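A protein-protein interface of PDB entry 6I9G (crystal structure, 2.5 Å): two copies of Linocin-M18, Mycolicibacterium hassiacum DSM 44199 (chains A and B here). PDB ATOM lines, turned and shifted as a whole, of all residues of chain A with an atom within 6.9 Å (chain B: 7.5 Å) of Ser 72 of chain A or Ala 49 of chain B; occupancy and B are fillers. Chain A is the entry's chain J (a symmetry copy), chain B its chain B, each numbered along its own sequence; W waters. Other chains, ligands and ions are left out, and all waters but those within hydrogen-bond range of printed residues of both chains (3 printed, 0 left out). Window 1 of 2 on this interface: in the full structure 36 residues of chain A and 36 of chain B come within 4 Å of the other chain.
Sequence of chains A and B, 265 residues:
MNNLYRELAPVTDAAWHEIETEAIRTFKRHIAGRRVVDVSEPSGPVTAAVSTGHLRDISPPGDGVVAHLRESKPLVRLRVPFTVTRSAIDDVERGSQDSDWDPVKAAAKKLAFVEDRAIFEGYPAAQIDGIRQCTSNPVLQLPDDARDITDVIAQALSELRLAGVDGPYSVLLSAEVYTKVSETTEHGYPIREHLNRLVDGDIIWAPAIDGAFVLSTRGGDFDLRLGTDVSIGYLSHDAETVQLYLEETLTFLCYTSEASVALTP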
ATOM      1  N   ALA A  48     -34.837  24.159 -15.388  1.00  0.00           N
ATOM      2  CA  ALA A  48     -35.278  24.942 -16.541  1.00  0.00           C
ATOM      3  C   ALA A  48     -35.326  24.156 -17.868  1.00  0.00           C
ATOM      4  O   ALA A  48     -35.985  24.589 -18.828  1.00  0.00           O
ATOM      5  CB  ALA A  48     -34.400  26.178 -16.687  1.00  0.00           C
ATOM      6  N   ALA A  49     -34.623  23.018 -17.919  1.00  0.00           N
ATOM      7  CA  ALA A  49     -34.406  22.285 -19.175  1.00  0.00           C
ATOM      8  C   ALA A  49     -34.067  20.833 -18.929  1.00  0.00           C
ATOM      9  O   ALA A  49     -33.670  20.465 -17.829  1.00  0.00           O
ATOM     10  CB  ALA A  49     -33.296  22.935 -20.000  1.00  0.00           C
ATOM     11  N   VAL A  50     -34.218  20.016 -19.966  1.00  0.00           N
ATOM     12  CA  VAL A  50     -33.836  18.599 -19.921  1.00  0.00           C
ATOM     13  C   VAL A  50     -32.801  18.351 -21.019  1.00  0.00           C
ATOM     14  O   VAL A  50     -33.068  18.539 -22.206  1.00  0.00           O
ATOM     15  CB  VAL A  50     -35.055  17.653 -20.113  1.00  0.00           C
ATOM     16  CG1 VAL A  50     -34.591  16.223 -20.279  1.00  0.00           C
ATOM     17  CG2 VAL A  50     -35.998  17.742 -18.934  1.00  0.00           C
ATOM     18  N   SER A  51     -31.609  17.940 -20.618  1.00  0.00           N
ATOM     19  CA  SER A  51     -30.571  17.550 -21.560  1.00  0.00           C
ATOM     20  C   SER A  51     -31.037  16.396 -22.455  1.00  0.00           C
ATOM     21  O   SER A  51     -31.590  15.394 -21.973  1.00  0.00           O
ATOM     22  CB  SER A  51     -29.349  17.112 -20.780  1.00  0.00           C
ATOM     23  OG  SER A  51     -28.385  16.562 -21.646  1.00  0.00           O
ATOM     24  N   THR A  52     -30.822  16.548 -23.757  1.00  0.00           N
ATOM     25  CA  THR A  52     -31.143  15.486 -24.695  1.00  0.00           C
ATOM     26  C   THR A  52     -29.917  14.678 -25.087  1.00  0.00           C
ATOM     27  O   THR A  52     -30.036  13.723 -25.848  1.00  0.00           O
ATOM     28  CB  THR A  52     -31.755  16.021 -26.003  1.00  0.00           C
ATOM     29  OG1 THR A  52     -30.802  16.854 -26.665  1.00  0.00           O
ATOM     30  CG2 THR A  52     -33.031  16.797 -25.750  1.00  0.00           C
ATOM     31  N   GLY A  53     -28.743  15.092 -24.615  1.00  0.00           N
ATOM     32  CA  GLY A  53     -27.480  14.435 -24.959  1.00  0.00           C
ATOM     33  C   GLY A  53     -26.856  14.815 -26.295  1.00  0.00           C
ATOM     34  O   GLY A  53     -25.704  14.475 -26.554  1.00  0.00           O
ATOM     35  N   HIS A  54     -27.591  15.533 -27.141  1.00  0.00           N
ATOM     36  CA  HIS A  54     -27.130  15.842 -28.499  1.00  0.00           C
ATOM     37  C   HIS A  54     -26.284  17.110 -28.566  1.00  0.00           C
ATOM     38  O   HIS A  54     -26.302  17.935 -27.640  1.00  0.00           O
ATOM     39  CB  HIS A  54     -28.313  15.953 -29.472  1.00  0.00           C
ATOM     40  CG  HIS A  54     -29.248  14.783 -29.434  1.00  0.00           C
ATOM     41  ND1 HIS A  54     -28.825  13.480 -29.600  1.00  0.00           N
ATOM     42  CD2 HIS A  54     -30.589  14.720 -29.262  1.00  0.00           C
ATOM     43  CE1 HIS A  54     -29.860  12.664 -29.516  1.00  0.00           C
ATOM     44  NE2 HIS A  54     -30.943  13.392 -29.313  1.00  0.00           N
ATOM     45  N   LEU A  69     -22.951  23.433 -29.288  1.00  0.00           N
ATOM     46  CA  LEU A  69     -23.861  23.723 -28.170  1.00  0.00           C
ATOM     47  C   LEU A  69     -24.525  22.440 -27.685  1.00  0.00           C
ATOM     48  O   LEU A  69     -24.907  21.593 -28.497  1.00  0.00           O
ATOM     49  CB  LEU A  69     -24.928  24.736 -28.530  1.00  0.00           C
ATOM     50  CG  LEU A  69     -24.598  26.214 -28.413  1.00  0.00           C
ATOM     51  CD1 LEU A  69     -25.859  27.014 -28.725  1.00  0.00           C
ATOM     52  CD2 LEU A  69     -24.057  26.564 -27.039  1.00  0.00           C
ATOM     53  N   ARG A  70     -24.635  22.300 -26.365  1.00  0.00           N
ATOM     54  CA  ARG A  70     -25.349  21.183 -25.767  1.00  0.00           C
ATOM     55  C   ARG A  70     -26.823  21.461 -25.897  1.00  0.00           C
ATOM     56  O   ARG A  70     -27.300  22.500 -25.452  1.00  0.00           O
ATOM     57  CB  ARG A  70     -24.976  21.024 -24.288  1.00  0.00           C
ATOM     58  CG  ARG A  70     -23.525  20.629 -24.055  1.00  0.00           C
ATOM     59  CD  ARG A  70     -23.241  19.223 -24.576  1.00  0.00           C
ATOM     60  NE  ARG A  70     -24.238  18.304 -24.044  1.00  0.00           N
ATOM     61  CZ  ARG A  70     -24.059  17.537 -22.977  1.00  0.00           C
ATOM     62  NH1 ARG A  70     -22.898  17.536 -22.333  1.00  0.00           N
ATOM     63  NH2 ARG A  70     -25.049  16.773 -22.558  1.00  0.00           N
ATOM     64  N   GLU A  71     -27.540  20.532 -26.510  1.00  0.00           N
ATOM     65  CA  GLU A  71     -28.983  20.676 -26.689  1.00  0.00           C
ATOM     66  C   GLU A  71     -29.802  20.237 -25.475  1.00  0.00           C
ATOM     67  O   GLU A  71     -29.439  19.284 -24.773  1.00  0.00           O
ATOM     68  CB  GLU A  71     -29.436  19.877 -27.896  1.00  0.00           C
ATOM     69  CG  GLU A  71     -29.022  20.480 -29.219  1.00  0.00           C
ATOM     70  CD  GLU A  71     -29.640  19.745 -30.387  1.00  0.00           C
ATOM     71  OE1 GLU A  71     -30.363  18.736 -30.134  1.00  0.00           O
ATOM     72  OE2 GLU A  71     -29.404  20.183 -31.542  1.00  0.00           O
ATOM     73  N   SER A  72     -30.922  20.929 -25.255  1.00  0.00           N
ATOM     74  CA  SER A  72     -31.868  20.560 -24.199  1.00  0.00           C
ATOM     75  C   SER A  72     -33.312  20.914 -24.583  1.00  0.00           C
ATOM     76  O   SER A  72     -33.505  21.752 -25.453  1.00  0.00           O
ATOM     77  CB  SER A  72     -31.477  21.256 -22.890  1.00  0.00           C
ATOM     78  OG  SER A  72     -31.576  22.651 -23.019  1.00  0.00           O
ATOM     79  N   LYS A  73     -34.312  20.271 -23.962  1.00  0.00           N
ATOM     80  CA  LYS A  73     -35.713  20.716 -24.090  1.00  0.00           C
ATOM     81  C   LYS A  73     -36.055  21.604 -22.911  1.00  0.00           C
ATOM     82  O   LYS A  73     -35.794  21.214 -21.763  1.00  0.00           O
ATOM     83  CB  LYS A  73     -36.710  19.551 -24.126  1.00  0.00           C
ATOM     84  CG  LYS A  73     -36.708  18.734 -25.396  1.00  0.00           C
ATOM     85  CD  LYS A  73     -37.085  19.558 -26.622  1.00  0.00           C
ATOM     86  CE  LYS A  73     -36.722  18.815 -27.890  1.00  0.00           C
ATOM     87  NZ  LYS A  73     -36.433  19.809 -28.947  1.00  0.00           N
ATOM     88  N   PRO A  74     -36.649  22.790 -23.179  1.00  0.00           N
ATOM     89  CA  PRO A  74     -37.045  23.700 -22.109  1.00  0.00           C
ATOM     90  C   PRO A  74     -38.255  23.176 -21.359  1.00  0.00           C
ATOM     91  O   PRO A  74     -39.099  22.572 -21.968  1.00  0.00           O
ATOM     92  CB  PRO A  74     -37.439  24.972 -22.871  1.00  0.00           C
ATOM     93  CG  PRO A  74     -37.837  24.503 -24.221  1.00  0.00           C
ATOM     94  CD  PRO A  74     -36.873  23.385 -24.507  1.00  0.00           C
ATOM     95  N   GLN A 127     -42.239  23.664 -27.541  1.00  0.00           N
ATOM     96  CA  GLN A 127     -41.250  22.777 -28.160  1.00  0.00           C
ATOM     97  C   GLN A 127     -41.442  21.312 -27.790  1.00  0.00           C
ATOM     98  O   GLN A 127     -40.481  20.547 -27.755  1.00  0.00           O
ATOM     99  CB  GLN A 127     -39.823  23.245 -27.841  1.00  0.00           C
ATOM    100  CG  GLN A 127     -39.535  24.605 -28.434  1.00  0.00           C
ATOM    101  CD  GLN A 127     -38.219  25.182 -27.990  1.00  0.00           C
ATOM    102  OE1 GLN A 127     -37.238  24.462 -27.764  1.00  0.00           O
ATOM    103  NE2 GLN A 127     -38.183  26.504 -27.871  1.00  0.00           N
ATOM    104  N   LEU A 253     -40.962  14.359 -23.274  1.00  0.00           N
ATOM    105  CA  LEU A 253     -40.075  13.934 -24.349  1.00  0.00           C
ATOM    106  C   LEU A 253     -40.450  12.543 -24.807  1.00  0.00           C
ATOM    107  O   LEU A 253     -40.727  11.675 -23.965  1.00  0.00           O
ATOM    108  CB  LEU A 253     -38.614  13.930 -23.902  1.00  0.00           C
ATOM    109  CG  LEU A 253     -38.000  15.234 -23.389  1.00  0.00           C
ATOM    110  CD1 LEU A 253     -38.062  15.266 -21.868  1.00  0.00           C
ATOM    111  CD2 LEU A 253     -36.553  15.301 -23.839  1.00  0.00           C
ATOM    112  N   SER B  43     -20.244  19.352 -13.106  1.00  0.00           N
ATOM    113  CA  SER B  43     -21.482  18.653 -12.782  1.00  0.00           C
ATOM    114  C   SER B  43     -21.685  17.374 -13.585  1.00  0.00           C
ATOM    115  O   SER B  43     -22.658  16.664 -13.360  1.00  0.00           O
ATOM    116  CB  SER B  43     -22.681  19.562 -12.968  1.00  0.00           C
ATOM    117  OG  SER B  43     -22.690  20.088 -14.279  1.00  0.00           O
ATOM    118  N   VAL B  46     -23.811  14.998 -18.459  1.00  0.00           N
ATOM    119  CA  VAL B  46     -25.231  15.110 -18.800  1.00  0.00           C
ATOM    120  C   VAL B  46     -25.672  16.576 -18.870  1.00  0.00           C
ATOM    121  O   VAL B  46     -26.543  16.924 -19.668  1.00  0.00           O
ATOM    122  CB  VAL B  46     -26.130  14.271 -17.846  1.00  0.00           C
ATOM    123  CG1 VAL B  46     -27.618  14.421 -18.183  1.00  0.00           C
ATOM    124  CG2 VAL B  46     -25.720  12.802 -17.895  1.00  0.00           C
ATOM    125  N   THR B  47     -25.072  17.431 -18.045  1.00  0.00           N
ATOM    126  CA  THR B  47     -25.512  18.824 -17.937  1.00  0.00           C
ATOM    127  C   THR B  47     -25.462  19.540 -19.290  1.00  0.00           C
ATOM    128  O   THR B  47     -24.433  19.526 -19.974  1.00  0.00           O
ATOM    129  CB  THR B  47     -24.665  19.606 -16.922  1.00  0.00           C
ATOM    130  OG1 THR B  47     -24.576  18.865 -15.699  1.00  0.00           O
ATOM    131  CG2 THR B  47     -25.274  20.990 -16.660  1.00  0.00           C
ATOM    132  N   ALA B  48     -26.562  20.172 -19.673  1.00  0.00           N
ATOM    133  CA  ALA B  48     -26.622  20.797 -20.980  1.00  0.00           C
ATOM    134  C   ALA B  48     -26.922  22.278 -20.896  1.00  0.00           C
ATOM    135  O   ALA B  48     -26.648  23.023 -21.840  1.00  0.00           O
ATOM    136  CB  ALA B  48     -27.646  20.102 -21.858  1.00  0.00           C
ATOM    137  N   ALA B  49     -27.504  22.707 -19.780  1.00  0.00           N
ATOM    138  CA  ALA B  49     -27.931  24.093 -19.635  1.00  0.00           C
ATOM    139  C   ALA B  49     -27.858  24.555 -18.182  1.00  0.00           C
ATOM    140  O   ALA B  49     -27.804  23.735 -17.259  1.00  0.00           O
ATOM    141  CB  ALA B  49     -29.332  24.280 -20.204  1.00  0.00           C
ATOM    142  N   VAL B  50     -27.833  25.875 -17.998  1.00  0.00           N
ATOM    143  CA  VAL B  50     -27.887  26.502 -16.678  1.00  0.00           C
ATOM    144  C   VAL B  50     -29.213  27.250 -16.612  1.00  0.00           C
ATOM    145  O   VAL B  50     -29.508  28.076 -17.485  1.00  0.00           O
ATOM    146  CB  VAL B  50     -26.736  27.519 -16.492  1.00  0.00           C
ATOM    147  CG1 VAL B  50     -26.824  28.209 -15.137  1.00  0.00           C
ATOM    148  CG2 VAL B  50     -25.394  26.834 -16.646  1.00  0.00           C
ATOM    149  N   SER B  51     -30.020  26.965 -15.597  1.00  0.00           N
ATOM    150  CA  SER B  51     -31.246  27.726 -15.404  1.00  0.00           C
ATOM    151  C   SER B  51     -30.894  29.175 -15.084  1.00  0.00           C
ATOM    152  O   SER B  51     -29.995  29.405 -14.300  1.00  0.00           O
ATOM    153  CB  SER B  51     -32.029  27.160 -14.237  1.00  0.00           C
ATOM    154  OG  SER B  51     -33.118  28.020 -13.964  1.00  0.00           O
ATOM    155  N   THR B  52     -31.582  30.143 -15.681  1.00  0.00           N
ATOM    156  CA  THR B  52     -31.387  31.549 -15.305  1.00  0.00           C
ATOM    157  C   THR B  52     -32.498  31.984 -14.362  1.00  0.00           C
ATOM    158  O   THR B  52     -32.475  33.097 -13.846  1.00  0.00           O
ATOM    159  CB  THR B  52     -31.431  32.496 -16.523  1.00  0.00           C
ATOM    160  OG1 THR B  52     -32.747  32.475 -17.096  1.00  0.00           O
ATOM    161  CG2 THR B  52     -30.429  32.079 -17.566  1.00  0.00           C
ATOM    162  N   GLU B  71     -36.337  29.751 -19.102  1.00  0.00           N
ATOM    163  CA  GLU B  71     -35.085  30.140 -19.782  1.00  0.00           C
ATOM    164  C   GLU B  71     -33.854  29.502 -19.180  1.00  0.00           C
ATOM    165  O   GLU B  71     -33.745  29.370 -17.961  1.00  0.00           O
ATOM    166  CB  GLU B  71     -34.874  31.633 -19.715  1.00  0.00           C
ATOM    167  CG  GLU B  71     -35.866  32.421 -20.525  1.00  0.00           C
ATOM    168  CD  GLU B  71     -35.327  33.782 -20.912  1.00  0.00           C
ATOM    169  OE1 GLU B  71     -34.363  34.268 -20.244  1.00  0.00           O
ATOM    170  OE2 GLU B  71     -35.880  34.346 -21.890  1.00  0.00           O
ATOM    171  N   SER B  72     -32.907  29.147 -20.039  1.00  0.00           N
ATOM    172  CA  SER B  72     -31.638  28.599 -19.585  1.00  0.00           C
ATOM    173  C   SER B  72     -30.515  29.018 -20.534  1.00  0.00           C
ATOM    174  O   SER B  72     -30.781  29.407 -21.660  1.00  0.00           O
ATOM    175  CB  SER B  72     -31.721  27.076 -19.506  1.00  0.00           C
ATOM    176  OG  SER B  72     -31.949  26.520 -20.786  1.00  0.00           O
ATOM    177  N   LYS B  73     -29.267  28.943 -20.088  1.00  0.00           N
ATOM    178  CA  LYS B  73     -28.158  29.169 -20.997  1.00  0.00           C
ATOM    179  C   LYS B  73     -27.521  27.828 -21.317  1.00  0.00           C
ATOM    180  O   LYS B  73     -27.208  27.052 -20.398  1.00  0.00           O
ATOM    181  CB  LYS B  73     -27.171  30.166 -20.406  1.00  0.00           C
ATOM    182  CG  LYS B  73     -27.764  31.577 -20.304  1.00  0.00           C
ATOM    183  CD  LYS B  73     -27.348  32.515 -21.442  1.00  0.00           C
ATOM    184  CE  LYS B  73     -25.835  32.724 -21.361  1.00  0.00           C
ATOM    185  NZ  LYS B  73     -25.434  34.151 -21.499  1.00  0.00           N
ATOM    186  N   PRO B  74     -27.373  27.521 -22.623  1.00  0.00           N
ATOM    187  CA  PRO B  74     -26.765  26.263 -23.054  1.00  0.00           C
ATOM    188  C   PRO B  74     -25.273  26.241 -22.762  1.00  0.00           C
ATOM    189  O   PRO B  74     -24.604  27.274 -22.840  1.00  0.00           O
ATOM    190  CB  PRO B  74     -26.996  26.250 -24.568  1.00  0.00           C
ATOM    191  CG  PRO B  74     -27.227  27.671 -24.948  1.00  0.00           C
ATOM    192  CD  PRO B  74     -27.824  28.355 -23.759  1.00  0.00           C
ATOM    193  N   LEU B  75     -24.758  25.065 -22.417  1.00  0.00           N
ATOM    194  CA  LEU B  75     -23.329  24.884 -22.225  1.00  0.00           C
ATOM    195  C   LEU B  75     -22.727  24.676 -23.589  1.00  0.00           C
ATOM    196  O   LEU B  75     -23.402  24.159 -24.483  1.00  0.00           O
ATOM    197  CB  LEU B  75     -23.070  23.661 -21.362  1.00  0.00           C
ATOM    198  CG  LEU B  75     -22.936  23.914 -19.867  1.00  0.00           C
ATOM    199  CD1 LEU B  75     -24.175  24.615 -19.356  1.00  0.00           C
ATOM    200  CD2 LEU B  75     -22.719  22.599 -19.128  1.00  0.00           C
ATOM    201  N   ARG B 225     -19.685  28.122 -15.158  1.00  0.00           N
ATOM    202  CA  ARG B 225     -20.246  26.807 -14.842  1.00  0.00           C
ATOM    203  C   ARG B 225     -19.619  25.710 -15.627  1.00  0.00           C
ATOM    204  O   ARG B 225     -19.753  25.694 -16.851  1.00  0.00           O
ATOM    205  CB  ARG B 225     -21.703  26.731 -15.240  1.00  0.00           C
ATOM    206  CG  ARG B 225     -22.634  27.377 -14.274  1.00  0.00           C
ATOM    207  CD  ARG B 225     -22.593  26.843 -12.853  1.00  0.00           C
ATOM    208  NE  ARG B 225     -23.572  27.688 -12.193  1.00  0.00           N
ATOM    209  CZ  ARG B 225     -24.845  27.358 -12.053  1.00  0.00           C
ATOM    210  NH1 ARG B 225     -25.269  26.156 -12.436  1.00  0.00           N
ATOM    211  NH2 ARG B 225     -25.685  28.218 -11.502  1.00  0.00           N
ATOM    212  N   THR B 251     -20.149  27.031 -19.561  1.00  0.00           N
ATOM    213  CA  THR B 251     -20.647  28.310 -20.008  1.00  0.00           C
ATOM    214  C   THR B 251     -20.320  29.369 -18.968  1.00  0.00           C
ATOM    215  O   THR B 251     -19.795  29.085 -17.872  1.00  0.00           O
ATOM    216  CB  THR B 251     -22.152  28.290 -20.356  1.00  0.00           C
ATOM    217  OG1 THR B 251     -22.507  29.521 -20.990  1.00  0.00           O
ATOM    218  CG2 THR B 251     -22.995  28.126 -19.112  1.00  0.00           C
HETATM  219  O   HOH W   1     -21.920  18.701 -19.491  1.00  0.00           O
HETATM  220  O   HOH W   2     -29.029  23.540 -23.699  1.00  0.00           O
HETATM  221  O   HOH W   3     -34.541  25.953 -20.882  1.00  0.00           O
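Of the printed residues of chain B, Ala 48 of chain A touches Ser 51 (3.5 Å), Glu 71 (3.5 Å) and Ser 72 (3.99 Å). Of the printed residues of chain B, Ser 51 of chain A touches Val 46 (2.7 Å) and Ala 48 (3.6 Å). Ser 72 of chain A touches just one residue of chain B: Ala 49 (3.95 Å). Printed residues of chain A within 4 Å of Thr 47 of chain B: Arg 70. Ala 49 of chain B touches just one residue of chain A: Ser 72 (3.95 Å). Thr 52 of chain B touches none of the printed residues of chain A. Of the printed residues of chain A, Pro 74 of chain B touches Leu 69 and Arg 70. Of the printed residues of chain A, Leu 75 of chain B touches Leu 69 and Arg 70. The nearest residue of chain B that does not touch Ser 72 of chain A is Ala 48 of chain B (4.1 Å). The nearest residue of chain A that does not touch Ala 49 of chain B is Ala 49 of chain A (4.2 Å). The nearest printed residue of chain B that does not touch Leu 69 of chain A is Ala 48 of chain B (6.2 Å).
The backbone carbonyl oxygen (O) of Ala 48 of chain B sits at hydrogen-bond distance from the backbone NH (N) of Leu 75 of chain B (2.8 Å). OG of Ser 51 of chain A sits at hydrogen-bond distance from N of Gly 53 of chain A. The side-chain hydroxyl of Ser 51 of chain A is in hydrogen-bond range of the guanidinium group of Arg 70 of chain A (3.5 Å). N of Glu 71 of chain A sits at hydrogen-bond distance from O of His 54 of chain A (3.1 Å). The backbone NH of Thr 52 of chain B lies within hydrogen-bond range of the backbone carbonyl oxygen of Glu 71 of chain B (3.2 Å). The side-chain hydroxyl (OG) of Ser 43 of chain B lies within hydrogen-bond range of the side-chain hydroxyl (OG1) of Thr 47 of chain B (2.7 Å).
Among the printed residues, merely in contact across the chains: Ala 48 of chain A with Glu 71 of chain B (3.5 Å), Glu 71 of chain A with Ala 48 of chain B (3.5 Å), Ala 48 of chain A with Ser 51 of chain B (3.5 Å), Leu 69 of chain A with Leu 75 of chain B (3.6 Å), Arg 70 of chain A with Ala 48 of chain B (3.6 Å), Ser 51 of chain A with Ala 48 of chain B (3.6 Å), Leu 69 of chain A with Pro 74 of chain B (3.9 Å), Arg 70 of chain A with Pro 74 of chain B (3.9 Å), Ala 49 of chain A with Ser 72 of chain B (3.9 Å), Ser 72 of chain A with Ala 49 of chain B (3.95 Å) and Ala 48 of chain A with Ser 72 of chain B (3.99 Å).
Hydrophobic or aromatic side chains of chain B within 4 Å of the printed part of chain A: Ala 48, Ala 49 and Pro 74. Of the 15 printed residues of chain A, 7 touch a printed residue of chain B. Printed residues of chain A that touch a printed residue of chain B: Ala 48, Ala 49, Ser 51, Leu 69, Arg 70, Glu 71 and Ser 72. Among the printed residues, 15 pairs touch across the chains. Among the printed residues, no Asp or Glu carboxylate lies within 4 Å of a Lys or Arg side-chain nitrogen of the other chain.
Water W3 lies within hydrogen-bond range of OG of Ser 72 of chain B (2.7 Å) and O of Ala 48 of chain A (2.9 Å). Water W2 lies within hydrogen-bond range of O of Arg 70 of chain A (2.7 Å), OG of Ser 72 of chain A (2.8 Å) and O of Ala 48 of chain B (3.1 Å). Water W1 bridges the backbone carbonyl oxygen (O) of Thr 47 of chain B (2.7 Å) and the guanidinium group (NH1) of Arg 70 of chain A (3.2 Å).
Ala 48 of chain A touches Ser 51 of chain B, and with the chains exchanged Ser 51 of chain A touches Ala 48 of chain B. Ala 48 of chain A touches Glu 71 of chain B, and with the chains exchanged Glu 71 of chain A touches Ala 48 of chain B. Ala 48 of chain A touches Ser 72 of chain B, but with the chains exchanged Ser 72 of chain A does not touch Ala 48 of chain B (4.1 Å). Ala 49 of chain A touches Ser 72 of chain B, and with the chains exchanged Ser 72 of chain A touches Ala 49 of chain B. 9 positions are printed for both chains. Of the 15 pairs that touch across the chains among the printed residues, 6 have their exchanged pair printed and touching as well.
O of Thr 47 of chain B lies within hydrogen-bond range of NH1 of Arg 70 of chain A, at 3.4 Å. The backbone NH of Arg 70 of chain A sits at hydrogen-bond distance from the backbone carbonyl oxygen of Leu 75 of chain B (2.9 Å). The backbone carbonyl oxygen (O) of Val 46 of chain B sits at hydrogen-bond distance from the side-chain hydroxyl (OG) of Ser 51 of chain A (2.7 Å). The guanidinium group of Arg 70 of chain A lies within hydrogen-bond range of the backbone carbonyl oxygen of Val 46 of chain B, at 3.3 Å.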
